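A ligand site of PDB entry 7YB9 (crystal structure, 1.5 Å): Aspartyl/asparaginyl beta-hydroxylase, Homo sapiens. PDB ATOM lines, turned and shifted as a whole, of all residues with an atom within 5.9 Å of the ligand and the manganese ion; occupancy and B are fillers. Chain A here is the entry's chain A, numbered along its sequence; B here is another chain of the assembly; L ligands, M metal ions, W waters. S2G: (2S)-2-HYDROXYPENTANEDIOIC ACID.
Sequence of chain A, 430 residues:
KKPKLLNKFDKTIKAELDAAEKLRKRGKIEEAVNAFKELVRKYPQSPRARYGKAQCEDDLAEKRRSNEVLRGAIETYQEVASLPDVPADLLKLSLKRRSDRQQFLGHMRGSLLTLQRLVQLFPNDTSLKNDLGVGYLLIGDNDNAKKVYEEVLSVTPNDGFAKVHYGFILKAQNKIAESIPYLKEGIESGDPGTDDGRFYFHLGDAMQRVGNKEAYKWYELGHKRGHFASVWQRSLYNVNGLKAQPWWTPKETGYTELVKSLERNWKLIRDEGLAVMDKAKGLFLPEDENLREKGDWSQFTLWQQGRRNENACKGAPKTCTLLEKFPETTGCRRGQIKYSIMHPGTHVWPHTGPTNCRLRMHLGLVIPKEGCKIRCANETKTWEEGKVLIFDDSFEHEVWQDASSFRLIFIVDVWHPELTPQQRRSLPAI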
ATOM      1  N   LEU A 291     -15.539  -2.074 -12.480  1.00  0.00           N
ATOM      2  CA  LEU A 291     -16.069  -0.961 -11.700  1.00  0.00           C
ATOM      3  C   LEU A 291     -16.213   0.335 -12.493  1.00  0.00           C
ATOM      4  O   LEU A 291     -16.730   1.323 -11.939  1.00  0.00           O
ATOM      5  CB  LEU A 291     -15.163  -0.689 -10.502  1.00  0.00           C
ATOM      6  CG  LEU A 291     -15.155  -1.854  -9.526  1.00  0.00           C
ATOM      7  CD1 LEU A 291     -14.114  -1.617  -8.457  1.00  0.00           C
ATOM      8  CD2 LEU A 291     -16.547  -2.038  -8.912  1.00  0.00           C
ATOM      9  N   TRP A 297      -8.273   4.006 -15.917  1.00  0.00           N
ATOM     10  CA  TRP A 297      -7.975   3.965 -14.494  1.00  0.00           C
ATOM     11  C   TRP A 297      -7.060   2.779 -14.288  1.00  0.00           C
ATOM     12  O   TRP A 297      -7.418   1.651 -14.633  1.00  0.00           O
ATOM     13  CB  TRP A 297      -9.261   3.775 -13.700  1.00  0.00           C
ATOM     14  CG  TRP A 297      -9.205   3.705 -12.301  1.00  0.00           C
ATOM     15  CD1 TRP A 297      -8.234   4.164 -11.442  1.00  0.00           C
ATOM     16  CD2 TRP A 297     -10.196   3.066 -11.481  1.00  0.00           C
ATOM     17  NE1 TRP A 297      -8.592   3.866 -10.134  1.00  0.00           N
ATOM     18  CE2 TRP A 297      -9.781   3.176 -10.145  1.00  0.00           C
ATOM     19  CE3 TRP A 297     -11.406   2.435 -11.758  1.00  0.00           C
ATOM     20  CZ2 TRP A 297     -10.521   2.674  -9.099  1.00  0.00           C
ATOM     21  CZ3 TRP A 297     -12.130   1.958 -10.745  1.00  0.00           C
ATOM     22  CH2 TRP A 297     -11.701   2.058  -9.433  1.00  0.00           C
ATOM     23  N   GLN A 299      -3.754   1.015 -11.572  1.00  0.00           N
ATOM     24  CA  GLN A 299      -3.169   1.000 -10.248  1.00  0.00           C
ATOM     25  C   GLN A 299      -1.840   0.252 -10.237  1.00  0.00           C
ATOM     26  O   GLN A 299      -1.644  -0.723 -10.938  1.00  0.00           O
ATOM     27  CB  GLN A 299      -4.134   0.380  -9.213  1.00  0.00           C
ATOM     28  CG  GLN A 299      -5.503   1.069  -9.239  1.00  0.00           C
ATOM     29  CD  GLN A 299      -6.437   0.625  -8.135  1.00  0.00           C
ATOM     30  OE1 GLN A 299      -6.670  -0.573  -7.944  1.00  0.00           O
ATOM     31  NE2 GLN A 299      -6.990   1.597  -7.402  1.00  0.00           N
ATOM     32  N   SER A 340      -2.826   5.039  -7.571  1.00  0.00           N
ATOM     33  CA  SER A 340      -3.964   4.998  -8.485  1.00  0.00           C
ATOM     34  C   SER A 340      -4.019   6.230  -9.373  1.00  0.00           C
ATOM     35  O   SER A 340      -4.125   7.363  -8.871  1.00  0.00           O
ATOM     36  CB  SER A 340      -5.221   4.901  -7.679  1.00  0.00           C
ATOM     37  OG  SER A 340      -6.344   4.676  -8.503  1.00  0.00           O
ATOM     38  N   ILE A 341      -4.007   5.991 -10.683  1.00  0.00           N
ATOM     39  CA  ILE A 341      -4.031   7.053 -11.697  1.00  0.00           C
ATOM     40  C   ILE A 341      -5.348   6.974 -12.450  1.00  0.00           C
ATOM     41  O   ILE A 341      -5.816   5.893 -12.820  1.00  0.00           O
ATOM     42  CB  ILE A 341      -2.814   7.006 -12.630  1.00  0.00           C
ATOM     43  CG1 ILE A 341      -2.800   8.332 -13.444  1.00  0.00           C
ATOM     44  CG2 ILE A 341      -2.861   5.763 -13.476  1.00  0.00           C
ATOM     45  CD1 ILE A 341      -1.546   8.584 -14.273  1.00  0.00           C
ATOM     46  N   MET A 342      -6.020   8.117 -12.582  1.00  0.00           N
ATOM     47  CA  MET A 342      -7.321   8.205 -13.226  1.00  0.00           C
ATOM     48  C   MET A 342      -7.254   9.382 -14.222  1.00  0.00           C
ATOM     49  O   MET A 342      -6.707  10.439 -13.887  1.00  0.00           O
ATOM     50  CB  MET A 342      -8.446   8.440 -12.238  1.00  0.00           C
ATOM     51  CG  MET A 342      -9.805   8.219 -12.825  1.00  0.00           C
ATOM     52  SD  MET A 342     -11.127   8.304 -11.601  1.00  0.00           S
ATOM     53  CE  MET A 342     -10.784   6.857 -10.585  1.00  0.00           C
ATOM     54  N   VAL A 348     -16.451   6.071 -12.184  1.00  0.00           N
ATOM     55  CA  VAL A 348     -16.425   4.811 -11.475  1.00  0.00           C
ATOM     56  C   VAL A 348     -17.841   4.641 -10.921  1.00  0.00           C
ATOM     57  O   VAL A 348     -18.348   5.501 -10.201  1.00  0.00           O
ATOM     58  CB  VAL A 348     -15.384   4.790 -10.348  1.00  0.00           C
ATOM     59  CG1 VAL A 348     -15.448   3.414  -9.656  1.00  0.00           C
ATOM     60  CG2 VAL A 348     -13.994   5.092 -10.868  1.00  0.00           C
ATOM     61  N   HIS A 351     -20.165   1.816  -5.806  1.00  0.00           N
ATOM     62  CA  HIS A 351     -19.767   0.472  -5.388  1.00  0.00           C
ATOM     63  C   HIS A 351     -19.316   0.478  -3.933  1.00  0.00           C
ATOM     64  O   HIS A 351     -19.045   1.518  -3.330  1.00  0.00           O
ATOM     65  CB  HIS A 351     -18.628  -0.101  -6.294  1.00  0.00           C
ATOM     66  CG  HIS A 351     -17.290   0.566  -6.072  1.00  0.00           C
ATOM     67  ND1 HIS A 351     -16.957   1.771  -6.660  1.00  0.00           N
ATOM     68  CD2 HIS A 351     -16.176   0.179  -5.390  1.00  0.00           C
ATOM     69  CE1 HIS A 351     -15.733   2.112  -6.312  1.00  0.00           C
ATOM     70  NE2 HIS A 351     -15.223   1.158  -5.576  1.00  0.00           N
ATOM     71  N   THR A 352     -19.196  -0.731  -3.411  1.00  0.00           N
ATOM     72  CA  THR A 352     -18.801  -1.002  -2.047  1.00  0.00           C
ATOM     73  C   THR A 352     -17.622  -1.959  -2.087  1.00  0.00           C
ATOM     74  O   THR A 352     -17.563  -2.825  -2.970  1.00  0.00           O
ATOM     75  CB  THR A 352     -20.050  -1.623  -1.344  1.00  0.00           C
ATOM     76  OG1 THR A 352     -20.826  -0.611  -0.712  1.00  0.00           O
ATOM     77  CG2 THR A 352     -19.613  -2.643  -0.393  1.00  0.00           C
ATOM     78  N   GLY A 353     -16.681  -1.792  -1.173  1.00  0.00           N
ATOM     79  CA  GLY A 353     -15.661  -2.807  -0.980  1.00  0.00           C
ATOM     80  C   GLY A 353     -16.191  -4.012  -0.211  1.00  0.00           C
ATOM     81  O   GLY A 353     -17.340  -4.052   0.227  1.00  0.00           O
ATOM     82  N   ARG A 360      -9.727   3.325   4.346  1.00  0.00           N
ATOM     83  CA  ARG A 360      -8.928   3.674   3.171  1.00  0.00           C
ATOM     84  C   ARG A 360      -8.517   5.120   3.229  1.00  0.00           C
ATOM     85  O   ARG A 360      -9.359   6.018   3.269  1.00  0.00           O
ATOM     86  CB  ARG A 360      -9.746   3.361   1.919  1.00  0.00           C
ATOM     87  CG  ARG A 360      -9.110   3.593   0.612  1.00  0.00           C
ATOM     88  CD  ARG A 360      -9.752   2.658  -0.434  1.00  0.00           C
ATOM     89  NE  ARG A 360      -9.136   1.339  -0.438  1.00  0.00           N
ATOM     90  CZ  ARG A 360      -9.324   0.430  -1.383  1.00  0.00           C
ATOM     91  NH1 ARG A 360     -10.106   0.716  -2.425  1.00  0.00           N
ATOM     92  NH2 ARG A 360      -8.665  -0.709  -1.345  1.00  0.00           N
ATOM     93  N   HIS A 362      -6.481   8.155   1.251  1.00  0.00           N
ATOM     94  CA  HIS A 362      -6.076   8.657  -0.043  1.00  0.00           C
ATOM     95  C   HIS A 362      -5.176   9.859   0.207  1.00  0.00           C
ATOM     96  O   HIS A 362      -5.632  10.829   0.819  1.00  0.00           O
ATOM     97  CB  HIS A 362      -7.291   9.161  -0.812  1.00  0.00           C
ATOM     98  CG  HIS A 362      -8.077   8.113  -1.498  1.00  0.00           C
ATOM     99  ND1 HIS A 362      -9.112   8.423  -2.344  1.00  0.00           N
ATOM    100  CD2 HIS A 362      -8.007   6.758  -1.469  1.00  0.00           C
ATOM    101  CE1 HIS A 362      -9.640   7.312  -2.837  1.00  0.00           C
ATOM    102  NE2 HIS A 362      -8.989   6.285  -2.321  1.00  0.00           N
ATOM    103  N   ILE A 374     -14.822  12.609  -5.262  1.00  0.00           N
ATOM    104  CA  ILE A 374     -15.236  11.309  -4.742  1.00  0.00           C
ATOM    105  C   ILE A 374     -16.378  11.492  -3.748  1.00  0.00           C
ATOM    106  O   ILE A 374     -16.272  12.257  -2.783  1.00  0.00           O
ATOM    107  CB  ILE A 374     -14.058  10.566  -4.069  1.00  0.00           C
ATOM    108  CG1 ILE A 374     -14.603   9.327  -3.364  1.00  0.00           C
ATOM    109  CG2 ILE A 374     -13.335  11.481  -3.070  1.00  0.00           C
ATOM    110  CD1 ILE A 374     -13.587   8.323  -2.942  1.00  0.00           C
ATOM    111  N   TRP A 383      -9.809  15.867  -3.415  1.00  0.00           N
ATOM    112  CA  TRP A 383      -8.442  15.664  -2.975  1.00  0.00           C
ATOM    113  C   TRP A 383      -7.673  16.969  -2.994  1.00  0.00           C
ATOM    114  O   TRP A 383      -8.048  17.929  -3.671  1.00  0.00           O
ATOM    115  CB  TRP A 383      -7.764  14.655  -3.887  1.00  0.00           C
ATOM    116  CG  TRP A 383      -8.382  13.285  -3.898  1.00  0.00           C
ATOM    117  CD1 TRP A 383      -8.130  12.281  -3.013  1.00  0.00           C
ATOM    118  CD2 TRP A 383      -9.352  12.779  -4.823  1.00  0.00           C
ATOM    119  NE1 TRP A 383      -8.851  11.190  -3.333  1.00  0.00           N
ATOM    120  CE2 TRP A 383      -9.599  11.454  -4.447  1.00  0.00           C
ATOM    121  CE3 TRP A 383     -10.014  13.308  -5.930  1.00  0.00           C
ATOM    122  CZ2 TRP A 383     -10.509  10.619  -5.146  1.00  0.00           C
ATOM    123  CZ3 TRP A 383     -10.885  12.476  -6.644  1.00  0.00           C
ATOM    124  CH2 TRP A 383     -11.144  11.157  -6.221  1.00  0.00           C
ATOM    125  N   PHE A 391     -11.748   7.405   4.361  1.00  0.00           N
ATOM    126  CA  PHE A 391     -13.149   6.997   4.256  1.00  0.00           C
ATOM    127  C   PHE A 391     -13.208   5.498   4.418  1.00  0.00           C
ATOM    128  O   PHE A 391     -12.224   4.768   4.202  1.00  0.00           O
ATOM    129  CB  PHE A 391     -13.772   7.461   2.921  1.00  0.00           C
ATOM    130  CG  PHE A 391     -13.228   6.750   1.664  1.00  0.00           C
ATOM    131  CD1 PHE A 391     -13.973   5.768   1.036  1.00  0.00           C
ATOM    132  CD2 PHE A 391     -12.038   7.140   1.088  1.00  0.00           C
ATOM    133  CE1 PHE A 391     -13.527   5.140  -0.128  1.00  0.00           C
ATOM    134  CE2 PHE A 391     -11.548   6.487  -0.085  1.00  0.00           C
ATOM    135  CZ  PHE A 391     -12.347   5.482  -0.678  1.00  0.00           C
ATOM    136  N   ASP A 393     -14.484   2.447   2.838  1.00  0.00           N
ATOM    137  CA  ASP A 393     -14.977   2.046   1.509  1.00  0.00           C
ATOM    138  C   ASP A 393     -15.954   0.851   1.557  1.00  0.00           C
ATOM    139  O   ASP A 393     -16.424   0.407   0.501  1.00  0.00           O
ATOM    140  CB  ASP A 393     -13.808   1.764   0.549  1.00  0.00           C
ATOM    141  CG  ASP A 393     -13.231   0.368   0.630  1.00  0.00           C
ATOM    142  OD1 ASP A 393     -13.150  -0.244   1.728  1.00  0.00           O
ATOM    143  OD2 ASP A 393     -12.794  -0.106  -0.434  1.00  0.00           O
ATOM    144  N   HIS A 397     -19.542   4.240  -2.564  1.00  0.00           N
ATOM    145  CA  HIS A 397     -18.811   5.413  -3.007  1.00  0.00           C
ATOM    146  C   HIS A 397     -18.641   5.396  -4.523  1.00  0.00           C
ATOM    147  O   HIS A 397     -18.818   4.371  -5.196  1.00  0.00           O
ATOM    148  CB  HIS A 397     -17.441   5.517  -2.311  1.00  0.00           C
ATOM    149  CG  HIS A 397     -16.591   4.311  -2.458  1.00  0.00           C
ATOM    150  ND1 HIS A 397     -16.805   3.154  -1.729  1.00  0.00           N
ATOM    151  CD2 HIS A 397     -15.548   4.043  -3.289  1.00  0.00           C
ATOM    152  CE1 HIS A 397     -15.929   2.236  -2.103  1.00  0.00           C
ATOM    153  NE2 HIS A 397     -15.155   2.756  -3.035  1.00  0.00           N
ATOM    154  N   VAL A 399     -16.773   7.809  -8.008  1.00  0.00           N
ATOM    155  CA  VAL A 399     -15.672   8.698  -8.359  1.00  0.00           C
ATOM    156  C   VAL A 399     -15.855   9.251  -9.754  1.00  0.00           C
ATOM    157  O   VAL A 399     -16.303   8.545 -10.673  1.00  0.00           O
ATOM    158  CB  VAL A 399     -14.312   7.993  -8.217  1.00  0.00           C
ATOM    159  CG1 VAL A 399     -13.194   8.908  -8.678  1.00  0.00           C
ATOM    160  CG2 VAL A 399     -14.056   7.593  -6.784  1.00  0.00           C
ATOM    161  N   ARG A 407      -4.935  12.467 -12.878  1.00  0.00           N
ATOM    162  CA  ARG A 407      -5.069  12.614 -11.427  1.00  0.00           C
ATOM    163  C   ARG A 407      -4.438  11.400 -10.774  1.00  0.00           C
ATOM    164  O   ARG A 407      -4.826  10.267 -11.042  1.00  0.00           O
ATOM    165  CB  ARG A 407      -6.529  12.697 -11.011  1.00  0.00           C
ATOM    166  CG  ARG A 407      -6.725  12.869  -9.499  1.00  0.00           C
ATOM    167  CD  ARG A 407      -7.691  11.844  -8.993  1.00  0.00           C
ATOM    168  NE  ARG A 407      -7.125  10.494  -9.135  1.00  0.00           N
ATOM    169  CZ  ARG A 407      -7.713   9.384  -8.725  1.00  0.00           C
ATOM    170  NH1 ARG A 407      -8.881   9.436  -8.160  1.00  0.00           N
ATOM    171  NH2 ARG A 407      -7.124   8.220  -8.896  1.00  0.00           N
ATOM    172  N   ILE A 409      -3.283   9.625  -7.141  1.00  0.00           N
ATOM    173  CA  ILE A 409      -3.374   9.531  -5.694  1.00  0.00           C
ATOM    174  C   ILE A 409      -2.579   8.300  -5.251  1.00  0.00           C
ATOM    175  O   ILE A 409      -2.169   7.450  -6.046  1.00  0.00           O
ATOM    176  CB  ILE A 409      -4.811   9.468  -5.179  1.00  0.00           C
ATOM    177  CG1 ILE A 409      -5.493   8.163  -5.670  1.00  0.00           C
ATOM    178  CG2 ILE A 409      -5.628  10.673  -5.707  1.00  0.00           C
ATOM    179  CD1 ILE A 409      -6.965   8.041  -5.139  1.00  0.00           C
ATOM    180  N   ILE A 411      -3.052   5.257  -2.284  1.00  0.00           N
ATOM    181  CA  ILE A 411      -4.102   4.618  -1.497  1.00  0.00           C
ATOM    182  C   ILE A 411      -3.426   3.748  -0.449  1.00  0.00           C
ATOM    183  O   ILE A 411      -2.595   2.877  -0.774  1.00  0.00           O
ATOM    184  CB  ILE A 411      -5.072   3.795  -2.373  1.00  0.00           C
ATOM    185  CG1 ILE A 411      -5.614   4.672  -3.525  1.00  0.00           C
ATOM    186  CG2 ILE A 411      -6.197   3.221  -1.496  1.00  0.00           C
ATOM    187  CD1 ILE A 411      -6.635   3.962  -4.419  1.00  0.00           C
ATOM    188  N   ASP B  18     -11.022  -3.875  -4.703  1.00  0.00           N
ATOM    189  CA  ASP B  18     -11.859  -2.687  -4.545  1.00  0.00           C
ATOM    190  C   ASP B  18     -13.322  -3.038  -4.445  1.00  0.00           C
ATOM    191  O   ASP B  18     -14.114  -2.251  -3.931  1.00  0.00           O
ATOM    192  CB  ASP B  18     -11.717  -1.764  -5.762  1.00  0.00           C
ATOM    193  CG  ASP B  18     -10.792  -0.654  -5.522  1.00  0.00           C
ATOM    194  OD1 ASP B  18      -9.751  -0.875  -4.785  1.00  0.00           O
ATOM    195  OD2 ASP B  18     -11.138   0.432  -6.042  1.00  0.00           O
HETATM  196  C1  S2G L   1     -11.179   3.406  -4.031  1.00  0.00           C
HETATM  197  C3  S2G L   1     -11.286   4.854  -6.025  1.00  0.00           C
HETATM  198  C4  S2G L   1      -9.776   5.025  -6.189  1.00  0.00           C
HETATM  199  C5  S2G L   1      -9.445   6.188  -7.050  1.00  0.00           C
HETATM  200  O2  S2G L   1     -11.943   2.793  -3.266  1.00  0.00           O
HETATM  201  O1  S2G L   1     -10.130   3.988  -3.586  1.00  0.00           O
HETATM  202  O3  S2G L   1     -12.860   3.025  -5.693  1.00  0.00           O
HETATM  203  O5  S2G L   1     -10.179   7.206  -7.066  1.00  0.00           O
HETATM  204  C2  S2G L   1     -11.538   3.435  -5.516  1.00  0.00           C
HETATM  205  O4  S2G L   1      -8.416   6.139  -7.740  1.00  0.00           O
HETATM  206 MN    MN M   1     -13.620   1.759  -4.164  1.00  0.00          MN
HETATM  207  O   HOH W   1      -8.830   1.669  -5.225  1.00  0.00           O
HETATM  208  O   HOH W   2     -13.598   0.272  -3.021  1.00  0.00           O
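The backbone carbonyl oxygen of Ser 340 is in hydrogen-bond range of the guanidinium group of Arg 407 (3.1 Å). ND1 of His 362 is in hydrogen-bond range of NE1 of Trp 383, at 3.0 Å. The backbone NH (N) of Arg 360 lies within hydrogen-bond range of the backbone carbonyl oxygen (O) of Phe 391 (2.9 Å). The backbone NH (N) of Ser 340 sits at hydrogen-bond distance from the backbone carbonyl oxygen (O) of Ile 409 (2.9 Å). N of Arg 407 sits at hydrogen-bond distance from O of Met 342, 2.9 Å away. The side-chain amide nitrogen (NE2) of Gln 299 is in hydrogen-bond range of the side-chain hydroxyl (OG) of Ser 340. NH1 of Arg 360 is in salt-bridge range of OD1 of Asp 18 of chain B, at 2.9 Å. The backbone carbonyl oxygen of Val 399 lies within hydrogen-bond range of the backbone NH of Val 348 (2.9 Å).
Merely in contact with the manganese ion: Asp 18 of chain B. Of the 22 residues printed, 3 come within 4 Å of the manganese ion. Along chain A the residues within 4 Å of the manganese ion span positions 351 to 397. The nearest printed residue that does not touch the manganese ion is Arg 360 (4.1 Å).
Water W2 bridges the backbone carbonyl oxygen of Asp 18 of chain B (2.7 Å) and the side-chain carboxylate of Asp 393 (2.7 Å). Water W1 lies within hydrogen-bond range of OD1 of Asp 18 of chain B, NE2 of Gln 299, O1 of the ligand and NH1 of Arg 360.
Water W2 binds the manganese ion, at 1.9 Å. An oxygen (O3) of the ligand is bound to the manganese ion (2.1 Å). NE2 of His 397 is bound to the manganese ion, 2.2 Å away. O2 of the ligand is bound to the manganese ion. NE2 of His 351 is bound to the manganese ion (2.2 Å).
Met 342 touches the ligand. Trp 383 touches the ligand (CZ2 to O5, 3.9 Å). CZ of Phe 391 touches O2 of the ligand, 3.8 Å away. Val 399 touches the ligand (CG1 to O5, 3.8 Å). Ile 409 touches the ligand. CD1 of Ile 411 touches O1 of the ligand, 3.6 Å away. Hydrophobic or aromatic side chains within 4 Å of the ligand: Trp 297, Met 342, His 351, His 362, Trp 383, Phe 391, His 397, Val 399, Ile 409 and Ile 411. Of the 22 residues printed, 14 come within 4 Å of the ligand.
An oxygen (O4) of the ligand lies within hydrogen-bond range of the indole nitrogen of Trp 297 (3.3 Å). An oxygen (O4) of the ligand is in hydrogen-bond range of the side-chain hydroxyl (OG) of Ser 340. A ring nitrogen (NE2) of His 362 lies within hydrogen-bond range of an oxygen (O1) of the ligand. NH1 of Arg 360 lies within salt-bridge range of O1 of the ligand, 3.5 Å away. O3 of the ligand sits close to OD2 of Asp 18 of chain B (3.1 Å). An oxygen (O4) of the ligand lies within salt-bridge range of the guanidinium group (NH2) of Arg 407, at 2.7 Å.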
